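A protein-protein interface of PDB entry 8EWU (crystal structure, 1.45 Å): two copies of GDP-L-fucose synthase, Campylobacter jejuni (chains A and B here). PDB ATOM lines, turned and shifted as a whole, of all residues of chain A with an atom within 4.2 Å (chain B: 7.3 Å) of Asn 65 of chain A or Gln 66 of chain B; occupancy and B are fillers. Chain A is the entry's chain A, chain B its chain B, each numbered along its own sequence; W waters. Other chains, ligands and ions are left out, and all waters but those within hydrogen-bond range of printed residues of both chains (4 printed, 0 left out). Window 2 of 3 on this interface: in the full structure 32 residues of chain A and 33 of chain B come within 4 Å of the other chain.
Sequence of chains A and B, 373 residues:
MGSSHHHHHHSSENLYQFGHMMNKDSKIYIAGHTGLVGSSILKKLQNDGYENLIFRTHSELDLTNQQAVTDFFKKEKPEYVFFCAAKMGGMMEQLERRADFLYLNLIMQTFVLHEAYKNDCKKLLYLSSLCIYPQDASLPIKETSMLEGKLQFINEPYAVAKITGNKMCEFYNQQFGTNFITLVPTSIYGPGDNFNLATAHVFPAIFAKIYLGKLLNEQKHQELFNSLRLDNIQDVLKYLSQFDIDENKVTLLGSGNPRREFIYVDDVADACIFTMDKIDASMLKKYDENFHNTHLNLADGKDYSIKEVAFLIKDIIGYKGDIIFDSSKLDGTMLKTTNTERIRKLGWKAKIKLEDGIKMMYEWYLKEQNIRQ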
ATOM      1  N   ASP A  62     -15.264   8.883   2.868  1.00  0.00           N
ATOM      2  CA  ASP A  62     -14.213   8.335   3.732  1.00  0.00           C
ATOM      3  C   ASP A  62     -13.996   9.328   4.877  1.00  0.00           C
ATOM      4  O   ASP A  62     -13.416  10.413   4.646  1.00  0.00           O
ATOM      5  CB  ASP A  62     -12.971   8.076   2.905  1.00  0.00           C
ATOM      6  CG  ASP A  62     -11.857   7.448   3.704  1.00  0.00           C
ATOM      7  OD1 ASP A  62     -11.992   7.303   4.934  1.00  0.00           O
ATOM      8  OD2 ASP A  62     -10.859   7.061   3.055  1.00  0.00           O
ATOM      9  N   LEU A  63     -14.449   8.963   6.083  1.00  0.00           N
ATOM     10  CA  LEU A  63     -14.392   9.865   7.238  1.00  0.00           C
ATOM     11  C   LEU A  63     -12.962   9.981   7.752  1.00  0.00           C
ATOM     12  O   LEU A  63     -12.793  10.814   8.627  1.00  0.00           O
ATOM     13  CB  LEU A  63     -15.335   9.406   8.344  1.00  0.00           C
ATOM     14  CG  LEU A  63     -16.805   9.413   7.934  1.00  0.00           C
ATOM     15  CD1 LEU A  63     -17.660   8.736   8.983  1.00  0.00           C
ATOM     16  CD2 LEU A  63     -17.305  10.829   7.713  1.00  0.00           C
ATOM     17  N   THR A  64     -11.988   9.301   7.161  1.00  0.00           N
ATOM     18  CA  THR A  64     -10.530   9.529   7.465  1.00  0.00           C
ATOM     19  C   THR A  64      -9.917  10.598   6.558  1.00  0.00           C
ATOM     20  O   THR A  64      -8.717  10.897   6.709  1.00  0.00           O
ATOM     21  CB  THR A  64      -9.673   8.265   7.374  1.00  0.00           C
ATOM     22  OG1 THR A  64      -9.649   7.756   6.035  1.00  0.00           O
ATOM     23  CG2 THR A  64     -10.171   7.220   8.351  1.00  0.00           C
ATOM     24  N   ASN A  65     -10.696  11.121   5.626  1.00  0.00           N
ATOM     25  CA  ASN A  65     -10.242  12.227   4.731  1.00  0.00           C
ATOM     26  C   ASN A  65     -10.802  13.547   5.241  1.00  0.00           C
ATOM     27  O   ASN A  65     -11.993  13.810   5.173  1.00  0.00           O
ATOM     28  CB  ASN A  65     -10.601  11.952   3.276  1.00  0.00           C
ATOM     29  CG  ASN A  65     -10.038  12.990   2.318  1.00  0.00           C
ATOM     30  OD1 ASN A  65     -10.539  14.103   2.223  1.00  0.00           O
ATOM     31  ND2 ASN A  65      -8.925  12.640   1.686  1.00  0.00           N
ATOM     32  N   GLN A  66      -9.911  14.375   5.767  1.00  0.00           N
ATOM     33  CA  GLN A  66     -10.309  15.639   6.402  1.00  0.00           C
ATOM     34  C   GLN A  66     -11.179  16.431   5.433  1.00  0.00           C
ATOM     35  O   GLN A  66     -12.238  16.960   5.836  1.00  0.00           O
ATOM     36  CB  GLN A  66      -9.054  16.407   6.806  1.00  0.00           C
ATOM     37  CG  GLN A  66      -9.385  17.711   7.516  1.00  0.00           C
ATOM     38  CD  GLN A  66      -8.139  18.498   7.797  1.00  0.00           C
ATOM     39  OE1 GLN A  66      -7.308  18.702   6.893  1.00  0.00           O
ATOM     40  NE2 GLN A  66      -8.006  18.917   9.047  1.00  0.00           N
ATOM     41  N   GLN A  67     -10.732  16.605   4.186  1.00  0.00           N
ATOM     42  CA  GLN A  67     -11.426  17.564   3.279  1.00  0.00           C
ATOM     43  C   GLN A  67     -12.806  16.997   2.864  1.00  0.00           C
ATOM     44  O   GLN A  67     -13.774  17.780   2.779  1.00  0.00           O
ATOM     45  CB  GLN A  67     -10.566  17.870   2.055  1.00  0.00           C
ATOM     46  CG  GLN A  67     -11.135  19.017   1.213  1.00  0.00           C
ATOM     47  CD  GLN A  67     -11.196  20.324   1.959  1.00  0.00           C
ATOM     48  OE1 GLN A  67     -10.204  20.756   2.584  1.00  0.00           O
ATOM     49  NE2 GLN A  67     -12.339  20.992   1.874  1.00  0.00           N
ATOM     50  N   ALA A  68     -12.907  15.708   2.691  1.00  0.00           N
ATOM     51  CA  ALA A  68     -14.188  15.043   2.344  1.00  0.00           C
ATOM     52  C   ALA A  68     -15.208  15.315   3.464  1.00  0.00           C
ATOM     53  O   ALA A  68     -16.374  15.629   3.162  1.00  0.00           O
ATOM     54  CB  ALA A  68     -14.010  13.575   2.058  1.00  0.00           C
ATOM     55  N   VAL A  69     -14.810  15.232   4.745  1.00  0.00           N
ATOM     56  CA  VAL A  69     -15.757  15.495   5.870  1.00  0.00           C
ATOM     57  C   VAL A  69     -16.105  16.970   5.885  1.00  0.00           C
ATOM     58  O   VAL A  69     -17.261  17.327   6.105  1.00  0.00           O
ATOM     59  CB  VAL A  69     -15.159  15.031   7.206  1.00  0.00           C
ATOM     60  CG1 VAL A  69     -16.097  15.343   8.354  1.00  0.00           C
ATOM     61  CG2 VAL A  69     -14.815  13.564   7.148  1.00  0.00           C
ATOM     62  N   PHE A 111     -12.681  14.816  12.979  1.00  0.00           N
ATOM     63  CA  PHE A 111     -13.193  15.561  11.803  1.00  0.00           C
ATOM     64  C   PHE A 111     -14.714  15.721  11.922  1.00  0.00           C
ATOM     65  O   PHE A 111     -15.225  16.846  11.739  1.00  0.00           O
ATOM     66  CB  PHE A 111     -12.857  14.860  10.499  1.00  0.00           C
ATOM     67  CG  PHE A 111     -11.399  14.669  10.203  1.00  0.00           C
ATOM     68  CD1 PHE A 111     -10.433  15.457  10.788  1.00  0.00           C
ATOM     69  CD2 PHE A 111     -11.003  13.615   9.405  1.00  0.00           C
ATOM     70  CE1 PHE A 111      -9.095  15.256  10.491  1.00  0.00           C
ATOM     71  CE2 PHE A 111      -9.666  13.415   9.113  1.00  0.00           C
ATOM     72  CZ  PHE A 111      -8.719  14.212   9.698  1.00  0.00           C
ATOM     73  N   ASP B  62       0.483  24.756   6.971  1.00  0.00           N
ATOM     74  CA  ASP B  62      -0.446  24.677   8.098  1.00  0.00           C
ATOM     75  C   ASP B  62      -0.570  23.212   8.457  1.00  0.00           C
ATOM     76  O   ASP B  62      -1.189  22.491   7.702  1.00  0.00           O
ATOM     77  CB  ASP B  62      -1.785  25.302   7.690  1.00  0.00           C
ATOM     78  CG  ASP B  62      -2.748  25.344   8.845  1.00  0.00           C
ATOM     79  OD1 ASP B  62      -2.474  24.710   9.880  1.00  0.00           O
ATOM     80  OD2 ASP B  62      -3.714  26.089   8.759  1.00  0.00           O
ATOM     81  N   LEU B  63      -0.005  22.824   9.607  1.00  0.00           N
ATOM     82  CA  LEU B  63       0.039  21.430  10.076  1.00  0.00           C
ATOM     83  C   LEU B  63      -1.329  20.939  10.549  1.00  0.00           C
ATOM     84  O   LEU B  63      -1.457  19.737  10.775  1.00  0.00           O
ATOM     85  CB  LEU B  63       1.103  21.285  11.160  1.00  0.00           C
ATOM     86  CG  LEU B  63       2.528  21.536  10.659  1.00  0.00           C
ATOM     87  CD1 LEU B  63       3.468  21.659  11.851  1.00  0.00           C
ATOM     88  CD2 LEU B  63       2.994  20.461   9.675  1.00  0.00           C
ATOM     89  N   THR B  64      -2.345  21.806  10.523  1.00  0.00           N
ATOM     90  CA  THR B  64      -3.739  21.419  10.765  1.00  0.00           C
ATOM     91  C   THR B  64      -4.439  21.020   9.469  1.00  0.00           C
ATOM     92  O   THR B  64      -5.594  20.617   9.556  1.00  0.00           O
ATOM     93  CB  THR B  64      -4.550  22.507  11.484  1.00  0.00           C
ATOM     94  OG1 THR B  64      -4.782  23.634  10.652  1.00  0.00           O
ATOM     95  CG2 THR B  64      -3.946  22.917  12.802  1.00  0.00           C
ATOM     96  N   ASN B  65      -3.746  21.045   8.334  1.00  0.00           N
ATOM     97  CA  ASN B  65      -4.354  20.650   7.047  1.00  0.00           C
ATOM     98  C   ASN B  65      -3.778  19.293   6.672  1.00  0.00           C
ATOM     99  O   ASN B  65      -2.583  19.184   6.366  1.00  0.00           O
ATOM    100  CB  ASN B  65      -4.157  21.734   5.981  1.00  0.00           C
ATOM    101  CG  ASN B  65      -4.851  21.348   4.679  1.00  0.00           C
ATOM    102  OD1 ASN B  65      -4.353  20.512   3.926  1.00  0.00           O
ATOM    103  ND2 ASN B  65      -6.075  21.861   4.494  1.00  0.00           N
ATOM    104  N   GLN B  66      -4.603  18.268   6.711  1.00  0.00           N
ATOM    105  CA  GLN B  66      -4.166  16.875   6.459  1.00  0.00           C
ATOM    106  C   GLN B  66      -3.408  16.802   5.140  1.00  0.00           C
ATOM    107  O   GLN B  66      -2.336  16.184   5.084  1.00  0.00           O
ATOM    108  CB  GLN B  66      -5.399  15.973   6.460  1.00  0.00           C
ATOM    109  CG  GLN B  66      -5.054  14.518   6.280  1.00  0.00           C
ATOM    110  CD  GLN B  66      -6.309  13.689   6.186  1.00  0.00           C
ATOM    111  OE1 GLN B  66      -7.213  13.990   5.422  1.00  0.00           O
ATOM    112  NE2 GLN B  66      -6.385  12.660   6.996  1.00  0.00           N
ATOM    113  N   GLN B  67      -3.986  17.339   4.056  1.00  0.00           N
ATOM    114  CA  GLN B  67      -3.410  17.139   2.696  1.00  0.00           C
ATOM    115  C   GLN B  67      -2.071  17.889   2.577  1.00  0.00           C
ATOM    116  O   GLN B  67      -1.136  17.371   1.970  1.00  0.00           O
ATOM    117  CB  GLN B  67      -4.388  17.606   1.614  1.00  0.00           C
ATOM    118  CG  GLN B  67      -3.900  17.245   0.197  1.00  0.00           C
ATOM    119  CD  GLN B  67      -3.817  15.751  -0.012  1.00  0.00           C
ATOM    120  OE1 GLN B  67      -4.746  15.010   0.313  1.00  0.00           O
ATOM    121  NE2 GLN B  67      -2.671  15.270  -0.474  1.00  0.00           N
ATOM    122  N   ALA B  68      -1.967  19.072   3.163  1.00  0.00           N
ATOM    123  CA  ALA B  68      -0.704  19.838   3.135  1.00  0.00           C
ATOM    124  C   ALA B  68       0.405  19.019   3.796  1.00  0.00           C
ATOM    125  O   ALA B  68       1.528  19.039   3.284  1.00  0.00           O
ATOM    126  CB  ALA B  68      -0.862  21.178   3.819  1.00  0.00           C
ATOM    127  N   VAL B  69       0.119  18.332   4.913  1.00  0.00           N
ATOM    128  CA  VAL B  69       1.150  17.538   5.618  1.00  0.00           C
ATOM    129  C   VAL B  69       1.557  16.336   4.772  1.00  0.00           C
ATOM    130  O   VAL B  69       2.760  16.068   4.636  1.00  0.00           O
ATOM    131  CB  VAL B  69       0.712  17.131   7.030  1.00  0.00           C
ATOM    132  CG1 VAL B  69       1.809  16.421   7.737  1.00  0.00           C
ATOM    133  CG2 VAL B  69       0.319  18.338   7.816  1.00  0.00           C
ATOM    134  N   THR B  70       0.587  15.692   4.159  1.00  0.00           N
ATOM    135  CA  THR B  70       0.851  14.580   3.234  1.00  0.00           C
ATOM    136  C   THR B  70       1.746  15.081   2.091  1.00  0.00           C
ATOM    137  O   THR B  70       2.726  14.397   1.751  1.00  0.00           O
ATOM    138  CB  THR B  70      -0.481  14.041   2.698  1.00  0.00           C
ATOM    139  OG1 THR B  70      -1.237  13.552   3.804  1.00  0.00           O
ATOM    140  CG2 THR B  70      -0.298  12.956   1.654  1.00  0.00           C
ATOM    141  N   ASP B  71       1.367  16.187   1.469  1.00  0.00           N
ATOM    142  CA  ASP B  71       2.107  16.720   0.294  1.00  0.00           C
ATOM    143  C   ASP B  71       3.544  17.034   0.697  1.00  0.00           C
ATOM    144  O   ASP B  71       4.478  16.685  -0.044  1.00  0.00           O
ATOM    145  CB  ASP B  71       1.381  17.925  -0.301  1.00  0.00           C
ATOM    146  CG  ASP B  71       0.068  17.612  -0.984  1.00  0.00           C
ATOM    147  OD1 ASP B  71      -0.183  16.444  -1.226  1.00  0.00           O
ATOM    148  OD2 ASP B  71      -0.738  18.559  -1.172  1.00  0.00           O
ATOM    149  N   PHE B  72       3.727  17.684   1.851  1.00  0.00           N
ATOM    150  CA  PHE B  72       5.055  18.092   2.318  1.00  0.00           C
ATOM    151  C   PHE B  72       5.934  16.867   2.540  1.00  0.00           C
ATOM    152  O   PHE B  72       7.087  16.846   2.086  1.00  0.00           O
ATOM    153  CB  PHE B  72       4.948  18.958   3.586  1.00  0.00           C
ATOM    154  CG  PHE B  72       6.256  19.140   4.299  1.00  0.00           C
ATOM    155  CD1 PHE B  72       7.173  20.094   3.886  1.00  0.00           C
ATOM    156  CD2 PHE B  72       6.604  18.325   5.359  1.00  0.00           C
ATOM    157  CE1 PHE B  72       8.376  20.246   4.557  1.00  0.00           C
ATOM    158  CE2 PHE B  72       7.819  18.472   6.011  1.00  0.00           C
ATOM    159  CZ  PHE B  72       8.706  19.428   5.616  1.00  0.00           C
ATOM    160  N   ILE B 107      -4.632  17.317  16.018  1.00  0.00           N
ATOM    161  CA  ILE B 107      -4.557  17.069  14.547  1.00  0.00           C
ATOM    162  C   ILE B 107      -3.139  17.333  14.041  1.00  0.00           C
ATOM    163  O   ILE B 107      -2.632  16.499  13.256  1.00  0.00           O
ATOM    164  CB  ILE B 107      -5.632  17.820  13.750  1.00  0.00           C
ATOM    165  CG1 ILE B 107      -5.549  19.336  13.795  1.00  0.00           C
ATOM    166  CG2 ILE B 107      -7.003  17.335  14.189  1.00  0.00           C
ATOM    167  CD1 ILE B 107      -6.684  20.002  13.028  1.00  0.00           C
ATOM    168  N   PHE B 111      -1.205  14.133  12.231  1.00  0.00           N
ATOM    169  CA  PHE B 111      -0.799  14.194  10.795  1.00  0.00           C
ATOM    170  C   PHE B 111       0.715  14.029  10.671  1.00  0.00           C
ATOM    171  O   PHE B 111       1.213  13.260   9.812  1.00  0.00           O
ATOM    172  CB  PHE B 111      -1.243  15.493  10.146  1.00  0.00           C
ATOM    173  CG  PHE B 111      -2.732  15.727  10.080  1.00  0.00           C
ATOM    174  CD1 PHE B 111      -3.645  14.697  10.183  1.00  0.00           C
ATOM    175  CD2 PHE B 111      -3.196  17.023  10.012  1.00  0.00           C
ATOM    176  CE1 PHE B 111      -5.004  14.941  10.118  1.00  0.00           C
ATOM    177  CE2 PHE B 111      -4.568  17.262   9.965  1.00  0.00           C
ATOM    178  CZ  PHE B 111      -5.448  16.213  10.063  1.00  0.00           C
ATOM    179  N   HIS B 114       1.816  10.335  11.683  1.00  0.00           N
ATOM    180  CA  HIS B 114       1.355   9.346  10.689  1.00  0.00           C
ATOM    181  C   HIS B 114       2.142   9.492   9.364  1.00  0.00           C
ATOM    182  O   HIS B 114       2.607   8.468   8.809  1.00  0.00           O
ATOM    183  CB  HIS B 114      -0.138   9.452  10.437  1.00  0.00           C
ATOM    184  CG  HIS B 114      -0.602   8.370   9.543  1.00  0.00           C
ATOM    185  ND1 HIS B 114      -0.671   7.078   9.956  1.00  0.00           N
ATOM    186  CD2 HIS B 114      -1.098   8.415   8.283  1.00  0.00           C
ATOM    187  CE1 HIS B 114      -1.108   6.333   8.945  1.00  0.00           C
ATOM    188  NE2 HIS B 114      -1.351   7.120   7.911  1.00  0.00           N
ATOM    189  N   GLU B 115       2.354  10.702   8.892  1.00  0.00           N
ATOM    190  CA  GLU B 115       3.076  10.882   7.612  1.00  0.00           C
ATOM    191  C   GLU B 115       4.554  10.559   7.789  1.00  0.00           C
ATOM    192  O   GLU B 115       5.177  10.145   6.806  1.00  0.00           O
ATOM    193  CB  GLU B 115       2.822  12.282   7.046  1.00  0.00           C
ATOM    194  CG  GLU B 115       1.395  12.491   6.624  1.00  0.00           C
ATOM    195  CD  GLU B 115       0.898  11.595   5.516  1.00  0.00           C
ATOM    196  OE1 GLU B 115       1.734  10.984   4.783  1.00  0.00           O
ATOM    197  OE2 GLU B 115      -0.312  11.498   5.410  1.00  0.00           O
HETATM  198  O   HOH W   1      -7.533  20.164   2.308  1.00  0.00           O
HETATM  199  O   HOH W   2      -6.814  18.325   4.215  1.00  0.00           O
HETATM  200  O   HOH W   3      -7.321  15.302   0.888  1.00  0.00           O
HETATM  201  O   HOH W   4      -7.887  15.795   3.487  1.00  0.00           O
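O of Thr 64 of chain A lies within hydrogen-bond range of NE2 of Gln 66 of chain B, 2.9 Å away.
The backbone carbonyl oxygen of Thr 64 of chain B sits at hydrogen-bond distance from the side-chain amide nitrogen of Gln 66 of chain A (3.0 Å).
OE1 of Gln 66 of chain A lies within hydrogen-bond range of N of Gln 66 of chain B.
OD1 of Asp 62 of chain A is in hydrogen-bond range of OG1 of Thr 64 of chain A, at 2.6 Å.
N of Gln 67 of chain A is in hydrogen-bond range of OD1 of Asn 65 of chain A, 3.2 Å away.
The backbone NH (N) of Ala 68 of chain A is in hydrogen-bond range of the side-chain amide oxygen (OD1) of Asn 65 of chain A (2.9 Å).
The side-chain carboxylate (OD1) of Asp 62 of chain B lies within hydrogen-bond range of the side-chain hydroxyl (OG1) of Thr 64 of chain B, 2.7 Å away.
The side-chain amide oxygen of Asn 65 of chain B sits at hydrogen-bond distance from the backbone NH of Gln 67 of chain B (3.2 Å).
The backbone carbonyl oxygen (O) of Gln 66 of chain B is in hydrogen-bond range of the side-chain hydroxyl (OG1) of Thr 70 of chain B, 3.1 Å away.
Among the printed residues, pairs that only touch across the chains: Gln 66 of chain A with Asn 65 of chain B (3.5 Å), Asn 65 of chain A with Gln 66 of chain B (3.6 Å), Phe 111 of chain A with Phe 111 of chain B (3.8 Å), Gln 66 of chain A with Phe 111 of chain B (3.9 Å) and Phe 111 of chain A with Gln 66 of chain B (3.9 Å).
Of the printed residues of chain B, Asn 65 of chain A touches Gln 66 (3.6 Å).
Of the printed residues of chain A, Gln 66 of chain B touches Thr 64, Asn 65, Gln 66 and Phe 111.
Of the printed residues of chain A, Phe 111 of chain B touches Gln 66 and Phe 111.
Of the printed residues of chain B, Gln 66 of chain A touches Thr 64 (3.0 Å), Asn 65 (3.5 Å), Gln 66 (2.7 Å) and Phe 111 (3.9 Å).
Of the printed residues of chain A, Asn 65 of chain B touches Gln 66 (3.5 Å).
Ala 68 of chain A touches none of the printed residues of chain B.
Asp 71 of chain B touches none of the printed residues of chain A.
The nearest printed residue of chain B that does not touch Thr 64 of chain A is Phe 111 of chain B (6.5 Å).
Of the 9 printed residues of chain A, 4 touch a printed residue of chain B.
Printed residues of chain B that touch a printed residue of chain A: Thr 64, Asn 65, Gln 66 and Phe 111.
Hydrophobic or aromatic side chains of chain B within 4 Å of the printed part of chain A: Phe 111.
Along chain B the printed residues that touch a printed residue of chain A span positions 64 to 111.
Among the printed residues, 8 pairs touch across the chains.
Among the printed residues, no Asp or Glu carboxylate lies within 4 Å of a Lys or Arg side-chain nitrogen of the other chain.
Thr 64 of chain A touches Gln 66 of chain B, and with the chains exchanged Gln 66 of chain A touches Thr 64 of chain B.
Gln 66 of chain B touches its own counterpart, Gln 66 of chain A.
Gln 66 of chain A touches Phe 111 of chain B, and with the chains exchanged Phe 111 of chain A touches Gln 66 of chain B.
Phe 111 of chain A touches its own counterpart, Phe 111 of chain B.
Positions printed for both chains: 62, 63, 64, 65, 66, 67, 68, 69 and 111.
Of the 8 pairs that touch across the chains among the printed residues, 8 have their exchanged pair printed and touching as well.
Water W3 lies within hydrogen-bond range of OE1 of Gln 67 of chain B and ND2 of Asn 65 of chain A.
Water W4 lies within hydrogen-bond range of the side-chain amide oxygen (OE1) of Gln 66 of chain B (2.7 Å), the backbone NH (N) of Gln 67 of chain A (3.0 Å), the backbone NH (N) of Gln 66 of chain A (3.4 Å) and the side-chain amide oxygen (OD1) of Asn 65 of chain A (3.4 Å).
Water W2 lies within hydrogen-bond range of OE1 of Gln 66 of chain A (2.7 Å), N of Gln 67 of chain B (3.0 Å), OD1 of Asn 65 of chain B (3.3 Å) and N of Gln 66 of chain B (3.3 Å).
Water W1 lies within hydrogen-bond range of the side-chain amide oxygen (OE1) of Gln 67 of chain A (2.7 Å) and the side-chain amide nitrogen (ND2) of Asn 65 of chain B (3.1 Å).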
